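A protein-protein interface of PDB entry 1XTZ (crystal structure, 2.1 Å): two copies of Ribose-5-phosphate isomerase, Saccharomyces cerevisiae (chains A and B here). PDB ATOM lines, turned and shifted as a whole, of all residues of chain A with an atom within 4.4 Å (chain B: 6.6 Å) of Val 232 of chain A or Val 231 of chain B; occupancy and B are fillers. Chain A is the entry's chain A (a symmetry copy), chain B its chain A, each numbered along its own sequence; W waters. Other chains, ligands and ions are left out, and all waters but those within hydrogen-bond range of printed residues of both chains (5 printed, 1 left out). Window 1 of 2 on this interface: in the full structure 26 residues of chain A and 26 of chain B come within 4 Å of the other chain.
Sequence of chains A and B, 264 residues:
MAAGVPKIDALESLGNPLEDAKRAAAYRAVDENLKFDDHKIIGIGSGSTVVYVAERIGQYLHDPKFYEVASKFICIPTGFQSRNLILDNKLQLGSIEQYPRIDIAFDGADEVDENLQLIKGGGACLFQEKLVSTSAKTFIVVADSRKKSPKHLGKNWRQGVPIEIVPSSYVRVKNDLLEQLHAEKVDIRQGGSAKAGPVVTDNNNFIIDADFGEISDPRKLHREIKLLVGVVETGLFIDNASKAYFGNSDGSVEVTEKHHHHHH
NZ of Lys 226 of chain A lies within hydrogen-bond range of O of Lys 226 of chain B.
NZ of Lys 226 of chain B sits at hydrogen-bond distance from O of Val 231 of chain A (3.1 Å).
The side-chain amino group of Lys 226 of chain A lies within hydrogen-bond range of the backbone carbonyl oxygen of Leu 228 of chain B.
The backbone carbonyl oxygen of Val 231 of chain B is in hydrogen-bond range of the side-chain amino group of Lys 226 of chain A (3.1 Å).
The backbone carbonyl oxygen (O) of Glu 164 of chain B is in hydrogen-bond range of the backbone NH (N) of Val 232 of chain B, at 2.7 Å.
The backbone carbonyl oxygen (O) of Val 166 of chain B sits at hydrogen-bond distance from the side-chain hydroxyl (OG) of Ser 169 of chain B (2.7 Å).
O of Gly 230 of chain B lies within hydrogen-bond range of N of Val 166 of chain B (2.8 Å).
The backbone carbonyl oxygen (O) of Glu 164 of chain A sits at hydrogen-bond distance from the backbone NH (N) of Val 232 of chain A.
N of Glu 164 of chain A is in hydrogen-bond range of O of Glu 233 of chain A, 2.8 Å away.
The backbone carbonyl oxygen (O) of Gly 230 of chain A sits at hydrogen-bond distance from the backbone NH (N) of Val 166 of chain A, 2.8 Å away.
Among the printed residues, merely in contact across the chains: Val 232 of chain A with Val 166 of chain B (3.6 Å), Val 166 of chain A with Val 232 of chain B (3.6 Å), Val 231 of chain A with Val 232 of chain B (3.7 Å), Val 232 of chain A with Val 231 of chain B (3.7 Å), Glu 233 of chain A with Val 229 of chain B (3.8 Å) and Lys 226 of chain A with Leu 227 of chain B (3.9 Å).
Of the printed residues of chain B, Val 232 of chain A touches Val 166 (3.6 Å) and Val 231 (3.7 Å).
Val 231 of chain B touches two residues of chain A.
Of the printed residues of chain A, Leu 227 of chain B touches Lys 226 (3.9 Å).
Of the printed residues of chain A, Leu 228 of chain B touches Lys 226 (3.0 Å).
Printed residues of chain B within 4 Å of Val 166 of chain A: Val 232 (3.6 Å).
Printed residues of chain A within 4 Å of Val 166 of chain B: Val 232.
Gly 230 of chain A touches none of the printed residues of chain B.
The nearest printed residue of chain A that does not touch Val 231 of chain B is Val 231 of chain A (4.8 Å).
Printed residues of chain A that touch a printed residue of chain B: Val 166, Lys 226, Val 231, Val 232 and Glu 233.
Hydrophobic or aromatic side chains of chain A within 4 Å of the printed part of chain B: Val 166 and Val 232.
Of the 19 printed residues of chain B, 7 touch a printed residue of chain A.
Printed residues of chain B that touch a printed residue of chain A: Val 166, Lys 226, Leu 227, Leu 228, Val 229, Val 231 and Val 232.
Hydrophobic or aromatic side chains of chain B within 4 Å of the printed part of chain A: Val 166, Leu 227, Val 229 and Val 232.
Among the printed residues, no Asp or Glu carboxylate lies within 4 Å of a Lys or Arg side-chain nitrogen of the other chain.
Val 166 of chain A touches Val 232 of chain B, and with the chains exchanged Val 232 of chain A touches Val 166 of chain B.
Lys 226 of chain B touches its own counterpart, Lys 226 of chain A.
Lys 226 of chain A touches Val 231 of chain B, and with the chains exchanged Val 231 of chain A touches Lys 226 of chain B.
Val 231 of chain A touches Val 232 of chain B, and with the chains exchanged Val 232 of chain A touches Val 231 of chain B.
Positions printed for both chains: 164, 165, 166, 205, 226, 230, 231, 232 and 233.
Of the 10 pairs that touch across the chains among the printed residues, 7 have their exchanged pair printed and touching as well.
Water W4 bridges OD1 of Asn 205 of chain A (2.7 Å) and ND2 of Asn 205 of chain B (2.8 Å).
Water W5 bridges OD1 of Asn 205 of chain B (2.7 Å) and ND2 of Asn 205 of chain A (2.8 Å).
Water W3 lies within hydrogen-bond range of the backbone carbonyl oxygen of Val 232 of chain B (2.8 Å), the side-chain carboxylate of Glu 233 of chain B (2.8 Å) and the backbone NH of Gly 230 of chain A (2.8 Å).
Water W1 lies within hydrogen-bond range of O of Val 232 of chain A (2.8 Å), OE1 of Glu 233 of chain A (2.8 Å) and N of Gly 230 of chain B (2.8 Å).
Water W2 lies within hydrogen-bond range of OE1 of Glu 233 of chain A and O of Leu 227 of chain B.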
ATOM      1  N   GLU A 164      -0.165  29.044   3.254  1.00  0.00           N
ATOM      2  CA  GLU A 164      -0.046  27.749   3.935  1.00  0.00           C
ATOM      3  C   GLU A 164       0.998  26.922   3.222  1.00  0.00           C
ATOM      4  O   GLU A 164       0.995  26.824   1.954  1.00  0.00           O
ATOM      5  CB  GLU A 164      -1.419  27.018   3.989  1.00  0.00           C
ATOM      6  CG  GLU A 164      -1.434  25.672   4.776  1.00  0.00           C
ATOM      7  CD  GLU A 164      -2.826  25.309   5.329  1.00  0.00           C
ATOM      8  OE1 GLU A 164      -3.722  26.160   5.211  1.00  0.00           O
ATOM      9  OE2 GLU A 164      -3.024  24.209   5.904  1.00  0.00           O
ATOM     10  N   ILE A 165       1.905  26.339   4.021  1.00  0.00           N
ATOM     11  CA  ILE A 165       3.048  25.610   3.464  1.00  0.00           C
ATOM     12  C   ILE A 165       3.282  24.223   4.118  1.00  0.00           C
ATOM     13  O   ILE A 165       2.992  24.010   5.295  1.00  0.00           O
ATOM     14  CB  ILE A 165       4.370  26.443   3.606  1.00  0.00           C
ATOM     15  CG1 ILE A 165       4.653  26.711   5.087  1.00  0.00           C
ATOM     16  CG2 ILE A 165       4.256  27.832   2.849  1.00  0.00           C
ATOM     17  CD1 ILE A 165       6.134  26.990   5.405  1.00  0.00           C
ATOM     18  N   VAL A 166       3.886  23.307   3.363  1.00  0.00           N
ATOM     19  CA  VAL A 166       4.290  22.007   3.933  1.00  0.00           C
ATOM     20  C   VAL A 166       5.368  22.301   4.996  1.00  0.00           C
ATOM     21  O   VAL A 166       6.251  23.115   4.752  1.00  0.00           O
ATOM     22  CB  VAL A 166       4.842  21.092   2.806  1.00  0.00           C
ATOM     23  CG1 VAL A 166       5.248  19.700   3.366  1.00  0.00           C
ATOM     24  CG2 VAL A 166       3.775  20.960   1.706  1.00  0.00           C
ATOM     25  N   ASN A 205      -0.300  21.924   8.515  1.00  0.00           N
ATOM     26  CA  ASN A 205       0.689  22.722   7.781  1.00  0.00           C
ATOM     27  C   ASN A 205       1.177  23.906   8.611  1.00  0.00           C
ATOM     28  O   ASN A 205       0.585  24.243   9.650  1.00  0.00           O
ATOM     29  CB  ASN A 205       0.113  23.182   6.423  1.00  0.00           C
ATOM     30  CG  ASN A 205      -0.135  21.996   5.466  1.00  0.00           C
ATOM     31  OD1 ASN A 205       0.699  21.078   5.384  1.00  0.00           O
ATOM     32  ND2 ASN A 205      -1.306  21.962   4.816  1.00  0.00           N
ATOM     33  N   LYS A 226       1.595  30.263  -5.635  1.00  0.00           N
ATOM     34  CA  LYS A 226       0.957  28.936  -5.692  1.00  0.00           C
ATOM     35  C   LYS A 226       1.831  27.913  -6.422  1.00  0.00           C
ATOM     36  O   LYS A 226       1.792  26.736  -6.071  1.00  0.00           O
ATOM     37  CB  LYS A 226      -0.438  29.033  -6.356  1.00  0.00           C
ATOM     38  CG  LYS A 226      -1.294  27.699  -6.389  1.00  0.00           C
ATOM     39  CD  LYS A 226      -1.719  27.286  -4.998  1.00  0.00           C
ATOM     40  CE  LYS A 226      -2.792  26.160  -5.061  1.00  0.00           C
ATOM     41  NZ  LYS A 226      -2.216  24.803  -5.378  1.00  0.00           N
ATOM     42  N   GLY A 230       6.449  23.712  -1.920  1.00  0.00           N
ATOM     43  CA  GLY A 230       6.202  23.904  -0.456  1.00  0.00           C
ATOM     44  C   GLY A 230       4.891  24.636  -0.204  1.00  0.00           C
ATOM     45  O   GLY A 230       4.305  24.503   0.881  1.00  0.00           O
ATOM     46  N   VAL A 231       4.433  25.411  -1.197  1.00  0.00           N
ATOM     47  CA  VAL A 231       3.210  26.177  -1.013  1.00  0.00           C
ATOM     48  C   VAL A 231       2.013  25.286  -1.221  1.00  0.00           C
ATOM     49  O   VAL A 231       1.889  24.650  -2.284  1.00  0.00           O
ATOM     50  CB  VAL A 231       3.125  27.412  -1.928  1.00  0.00           C
ATOM     51  CG1 VAL A 231       1.712  28.039  -1.872  1.00  0.00           C
ATOM     52  CG2 VAL A 231       4.196  28.412  -1.514  1.00  0.00           C
ATOM     53  N   VAL A 232       1.157  25.216  -0.202  1.00  0.00           N
ATOM     54  CA  VAL A 232      -0.124  24.478  -0.296  1.00  0.00           C
ATOM     55  C   VAL A 232      -1.262  25.374  -0.888  1.00  0.00           C
ATOM     56  O   VAL A 232      -1.958  25.008  -1.856  1.00  0.00           O
ATOM     57  CB  VAL A 232      -0.508  23.958   1.094  1.00  0.00           C
ATOM     58  CG1 VAL A 232      -1.955  23.380   1.101  1.00  0.00           C
ATOM     59  CG2 VAL A 232       0.527  22.936   1.605  1.00  0.00           C
ATOM     60  N   GLU A 233      -1.458  26.549  -0.297  1.00  0.00           N
ATOM     61  CA  GLU A 233      -2.466  27.473  -0.782  1.00  0.00           C
ATOM     62  C   GLU A 233      -2.125  28.869  -0.286  1.00  0.00           C
ATOM     63  O   GLU A 233      -1.436  29.013   0.711  1.00  0.00           O
ATOM     64  CB  GLU A 233      -3.878  27.000  -0.298  1.00  0.00           C
ATOM     65  CG  GLU A 233      -5.038  27.779  -0.839  1.00  0.00           C
ATOM     66  CD  GLU A 233      -4.987  27.913  -2.386  1.00  0.00           C
ATOM     67  OE1 GLU A 233      -5.352  26.934  -3.112  1.00  0.00           O
ATOM     68  OE2 GLU A 233      -4.544  28.995  -2.858  1.00  0.00           O
ATOM     69  N   ILE B 163      -0.243  12.705  -7.395  1.00  0.00           N
ATOM     70  CA  ILE B 163      -0.510  14.100  -7.045  1.00  0.00           C
ATOM     71  C   ILE B 163      -0.763  14.089  -5.544  1.00  0.00           C
ATOM     72  O   ILE B 163      -1.657  13.364  -5.068  1.00  0.00           O
ATOM     73  CB  ILE B 163      -1.753  14.731  -7.812  1.00  0.00           C
ATOM     74  CG1 ILE B 163      -1.617  14.602  -9.346  1.00  0.00           C
ATOM     75  CG2 ILE B 163      -1.926  16.281  -7.459  1.00  0.00           C
ATOM     76  CD1 ILE B 163      -2.943  14.890 -10.128  1.00  0.00           C
ATOM     77  N   GLU B 164      -0.002  14.896  -4.797  1.00  0.00           N
ATOM     78  CA  GLU B 164      -0.249  14.981  -3.352  1.00  0.00           C
ATOM     79  C   GLU B 164      -1.265  16.069  -3.098  1.00  0.00           C
ATOM     80  O   GLU B 164      -1.152  17.206  -3.655  1.00  0.00           O
ATOM     81  CB  GLU B 164       1.073  15.236  -2.572  1.00  0.00           C
ATOM     82  CG  GLU B 164       0.947  15.248  -1.018  1.00  0.00           C
ATOM     83  CD  GLU B 164       2.261  14.887  -0.301  1.00  0.00           C
ATOM     84  OE1 GLU B 164       3.207  14.507  -1.008  1.00  0.00           O
ATOM     85  OE2 GLU B 164       2.349  14.946   0.952  1.00  0.00           O
ATOM     86  N   ILE B 165      -2.270  15.729  -2.277  1.00  0.00           N
ATOM     87  CA  ILE B 165      -3.394  16.639  -2.038  1.00  0.00           C
ATOM     88  C   ILE B 165      -3.759  16.798  -0.538  1.00  0.00           C
ATOM     89  O   ILE B 165      -3.589  15.882   0.266  1.00  0.00           O
ATOM     90  CB  ILE B 165      -4.679  16.160  -2.801  1.00  0.00           C
ATOM     91  CG1 ILE B 165      -5.081  14.767  -2.308  1.00  0.00           C
ATOM     92  CG2 ILE B 165      -4.424  16.093  -4.365  1.00  0.00           C
ATOM     93  CD1 ILE B 165      -6.569  14.428  -2.521  1.00  0.00           C
ATOM     94  N   VAL B 166      -4.338  17.946  -0.190  1.00  0.00           N
ATOM     95  CA  VAL B 166      -4.859  18.142   1.177  1.00  0.00           C
ATOM     96  C   VAL B 166      -6.013  17.136   1.365  1.00  0.00           C
ATOM     97  O   VAL B 166      -6.826  16.976   0.462  1.00  0.00           O
ATOM     98  CB  VAL B 166      -5.353  19.606   1.342  1.00  0.00           C
ATOM     99  CG1 VAL B 166      -5.880  19.858   2.782  1.00  0.00           C
ATOM    100  CG2 VAL B 166      -4.198  20.562   0.996  1.00  0.00           C
ATOM    101  N   SER B 169      -9.760  17.763   0.395  1.00  0.00           N
ATOM    102  CA  SER B 169     -10.005  18.198  -0.962  1.00  0.00           C
ATOM    103  C   SER B 169     -10.149  17.067  -1.988  1.00  0.00           C
ATOM    104  O   SER B 169     -10.215  17.340  -3.174  1.00  0.00           O
ATOM    105  CB  SER B 169      -8.868  19.125  -1.429  1.00  0.00           C
ATOM    106  OG  SER B 169      -7.696  18.355  -1.738  1.00  0.00           O
ATOM    107  N   VAL B 173     -10.637  17.856  -5.905  1.00  0.00           N
ATOM    108  CA  VAL B 173      -9.483  17.726  -6.792  1.00  0.00           C
ATOM    109  C   VAL B 173      -9.814  16.715  -7.903  1.00  0.00           C
ATOM    110  O   VAL B 173      -9.504  16.944  -9.095  1.00  0.00           O
ATOM    111  CB  VAL B 173      -8.138  17.327  -6.035  1.00  0.00           C
ATOM    112  CG1 VAL B 173      -6.983  17.051  -7.099  1.00  0.00           C
ATOM    113  CG2 VAL B 173      -7.669  18.464  -5.102  1.00  0.00           C
ATOM    114  N   LEU B 177      -9.764  17.597 -11.838  1.00  0.00           N
ATOM    115  CA  LEU B 177      -8.865  16.864 -12.732  1.00  0.00           C
ATOM    116  C   LEU B 177      -9.666  16.279 -13.919  1.00  0.00           C
ATOM    117  O   LEU B 177      -9.220  16.343 -15.066  1.00  0.00           O
ATOM    118  CB  LEU B 177      -8.160  15.750 -11.945  1.00  0.00           C
ATOM    119  CG  LEU B 177      -7.058  16.182 -10.938  1.00  0.00           C
ATOM    120  CD1 LEU B 177      -6.666  14.935 -10.145  1.00  0.00           C
ATOM    121  CD2 LEU B 177      -5.870  16.739 -11.715  1.00  0.00           C
ATOM    122  N   ASN B 205      -0.716  14.016   3.984  1.00  0.00           N
ATOM    123  CA  ASN B 205      -1.592  14.289   2.838  1.00  0.00           C
ATOM    124  C   ASN B 205      -2.091  12.996   2.198  1.00  0.00           C
ATOM    125  O   ASN B 205      -1.580  11.902   2.488  1.00  0.00           O
ATOM    126  CB  ASN B 205      -0.871  15.189   1.809  1.00  0.00           C
ATOM    127  CG  ASN B 205      -0.599  16.603   2.366  1.00  0.00           C
ATOM    128  OD1 ASN B 205      -1.468  17.186   3.035  1.00  0.00           O
ATOM    129  ND2 ASN B 205       0.623  17.117   2.173  1.00  0.00           N
ATOM    130  N   GLU B 224      -0.869  23.356 -14.579  1.00  0.00           N
ATOM    131  CA  GLU B 224      -2.322  23.293 -14.441  1.00  0.00           C
ATOM    132  C   GLU B 224      -2.756  22.544 -13.199  1.00  0.00           C
ATOM    133  O   GLU B 224      -3.675  22.977 -12.492  1.00  0.00           O
ATOM    134  CB  GLU B 224      -2.935  22.686 -15.698  1.00  0.00           C
ATOM    135  CG  GLU B 224      -2.834  23.617 -16.928  1.00  0.00           C
ATOM    136  CD  GLU B 224      -3.227  22.897 -18.239  1.00  0.00           C
ATOM    137  OE1 GLU B 224      -3.151  21.648 -18.320  1.00  0.00           O
ATOM    138  OE2 GLU B 224      -3.593  23.589 -19.196  1.00  0.00           O
ATOM    139  N   ILE B 225      -2.124  21.412 -12.924  1.00  0.00           N
ATOM    140  CA  ILE B 225      -2.475  20.619 -11.732  1.00  0.00           C
ATOM    141  C   ILE B 225      -2.071  21.400 -10.473  1.00  0.00           C
ATOM    142  O   ILE B 225      -2.840  21.512  -9.524  1.00  0.00           O
ATOM    143  CB  ILE B 225      -1.740  19.280 -11.750  1.00  0.00           C
ATOM    144  CG1 ILE B 225      -2.158  18.482 -12.992  1.00  0.00           C
ATOM    145  CG2 ILE B 225      -1.971  18.519 -10.437  1.00  0.00           C
ATOM    146  CD1 ILE B 225      -1.333  17.139 -13.212  1.00  0.00           C
ATOM    147  N   LYS B 226      -0.878  21.990 -10.498  1.00  0.00           N
ATOM    148  CA  LYS B 226      -0.308  22.684  -9.331  1.00  0.00           C
ATOM    149  C   LYS B 226      -1.163  23.878  -8.902  1.00  0.00           C
ATOM    150  O   LYS B 226      -1.217  24.177  -7.711  1.00  0.00           O
ATOM    151  CB  LYS B 226       1.146  23.131  -9.622  1.00  0.00           C
ATOM    152  CG  LYS B 226       1.931  23.797  -8.416  1.00  0.00           C
ATOM    153  CD  LYS B 226       2.205  22.793  -7.320  1.00  0.00           C
ATOM    154  CE  LYS B 226       3.220  23.367  -6.288  1.00  0.00           C
ATOM    155  NZ  LYS B 226       2.605  24.363  -5.337  1.00  0.00           N
ATOM    156  N   LEU B 227      -1.850  24.536  -9.864  1.00  0.00           N
ATOM    157  CA  LEU B 227      -2.694  25.680  -9.539  1.00  0.00           C
ATOM    158  C   LEU B 227      -4.026  25.280  -8.908  1.00  0.00           C
ATOM    159  O   LEU B 227      -4.752  26.133  -8.411  1.00  0.00           O
ATOM    160  CB  LEU B 227      -2.984  26.554 -10.786  1.00  0.00           C
ATOM    161  CG  LEU B 227      -1.767  27.310 -11.319  1.00  0.00           C
ATOM    162  CD1 LEU B 227      -2.097  27.913 -12.740  1.00  0.00           C
ATOM    163  CD2 LEU B 227      -1.347  28.361 -10.263  1.00  0.00           C
ATOM    164  N   LEU B 228      -4.357  23.997  -8.938  1.00  0.00           N
ATOM    165  CA  LEU B 228      -5.646  23.593  -8.393  1.00  0.00           C
ATOM    166  C   LEU B 228      -5.749  23.738  -6.862  1.00  0.00           C
ATOM    167  O   LEU B 228      -4.777  23.493  -6.147  1.00  0.00           O
ATOM    168  CB  LEU B 228      -5.950  22.163  -8.804  1.00  0.00           C
ATOM    169  CG  LEU B 228      -6.100  21.774 -10.288  1.00  0.00           C
ATOM    170  CD1 LEU B 228      -6.359  20.299 -10.403  1.00  0.00           C
ATOM    171  CD2 LEU B 228      -7.237  22.566 -10.957  1.00  0.00           C
ATOM    172  N   VAL B 229      -6.941  24.125  -6.375  1.00  0.00           N
ATOM    173  CA  VAL B 229      -7.264  24.136  -4.938  1.00  0.00           C
ATOM    174  C   VAL B 229      -7.289  22.696  -4.384  1.00  0.00           C
ATOM    175  O   VAL B 229      -8.103  21.871  -4.833  1.00  0.00           O
ATOM    176  CB  VAL B 229      -8.629  24.862  -4.629  1.00  0.00           C
ATOM    177  CG1 VAL B 229      -8.863  24.936  -3.152  1.00  0.00           C
ATOM    178  CG2 VAL B 229      -8.627  26.301  -5.197  1.00  0.00           C
ATOM    179  N   GLY B 230      -6.384  22.404  -3.442  1.00  0.00           N
ATOM    180  CA  GLY B 230      -6.262  21.037  -2.844  1.00  0.00           C
ATOM    181  C   GLY B 230      -4.943  20.378  -3.225  1.00  0.00           C
ATOM    182  O   GLY B 230      -4.466  19.486  -2.508  1.00  0.00           O
ATOM    183  N   VAL B 231      -4.357  20.811  -4.350  1.00  0.00           N
ATOM    184  CA  VAL B 231      -3.117  20.197  -4.803  1.00  0.00           C
ATOM    185  C   VAL B 231      -1.955  20.770  -4.035  1.00  0.00           C
ATOM    186  O   VAL B 231      -1.767  21.999  -4.015  1.00  0.00           O
ATOM    187  CB  VAL B 231      -2.885  20.347  -6.317  1.00  0.00           C
ATOM    188  CG1 VAL B 231      -1.453  19.904  -6.698  1.00  0.00           C
ATOM    189  CG2 VAL B 231      -3.936  19.536  -7.064  1.00  0.00           C
ATOM    190  N   VAL B 232      -1.200  19.886  -3.381  1.00  0.00           N
ATOM    191  CA  VAL B 232       0.045  20.278  -2.679  1.00  0.00           C
ATOM    192  C   VAL B 232       1.276  20.269  -3.643  1.00  0.00           C
ATOM    193  O   VAL B 232       2.038  21.250  -3.755  1.00  0.00           O
ATOM    194  CB  VAL B 232       0.272  19.331  -1.495  1.00  0.00           C
ATOM    195  CG1 VAL B 232       1.681  19.546  -0.863  1.00  0.00           C
ATOM    196  CG2 VAL B 232      -0.856  19.469  -0.454  1.00  0.00           C
ATOM    197  N   GLU B 233       1.478  19.150  -4.334  1.00  0.00           N
ATOM    198  CA  GLU B 233       2.573  19.042  -5.281  1.00  0.00           C
ATOM    199  C   GLU B 233       2.261  17.920  -6.258  1.00  0.00           C
ATOM    200  O   GLU B 233       1.493  17.027  -5.940  1.00  0.00           O
ATOM    201  CB  GLU B 233       3.909  18.796  -4.501  1.00  0.00           C
ATOM    202  CG  GLU B 233       5.152  18.801  -5.337  1.00  0.00           C
ATOM    203  CD  GLU B 233       5.249  20.062  -6.239  1.00  0.00           C
ATOM    204  OE1 GLU B 233       5.628  21.166  -5.733  1.00  0.00           O
ATOM    205  OE2 GLU B 233       4.908  19.937  -7.446  1.00  0.00           O
ATOM    206  N   THR B 234       2.868  17.959  -7.449  1.00  0.00           N
ATOM    207  CA  THR B 234       2.678  16.910  -8.469  1.00  0.00           C
ATOM    208  C   THR B 234       3.909  15.990  -8.562  1.00  0.00           C
ATOM    209  O   THR B 234       5.035  16.410  -8.238  1.00  0.00           O
ATOM    210  CB  THR B 234       2.394  17.518  -9.871  1.00  0.00           C
ATOM    211  OG1 THR B 234       3.614  17.948 -10.498  1.00  0.00           O
ATOM    212  CG2 THR B 234       1.516  18.764  -9.752  1.00  0.00           C
HETATM  213  O   HOH W   1      -4.553  24.346  -2.520  1.00  0.00           O
HETATM  214  O   HOH W   2      -5.533  27.912  -5.708  1.00  0.00           O
HETATM  215  O   HOH W   3       4.645  22.023  -3.287  1.00  0.00           O
HETATM  216  O   HOH W   4       1.621  18.868   4.083  1.00  0.00           O
HETATM  217  O   HOH W   5      -2.382  19.480   4.189  1.00  0.00           O
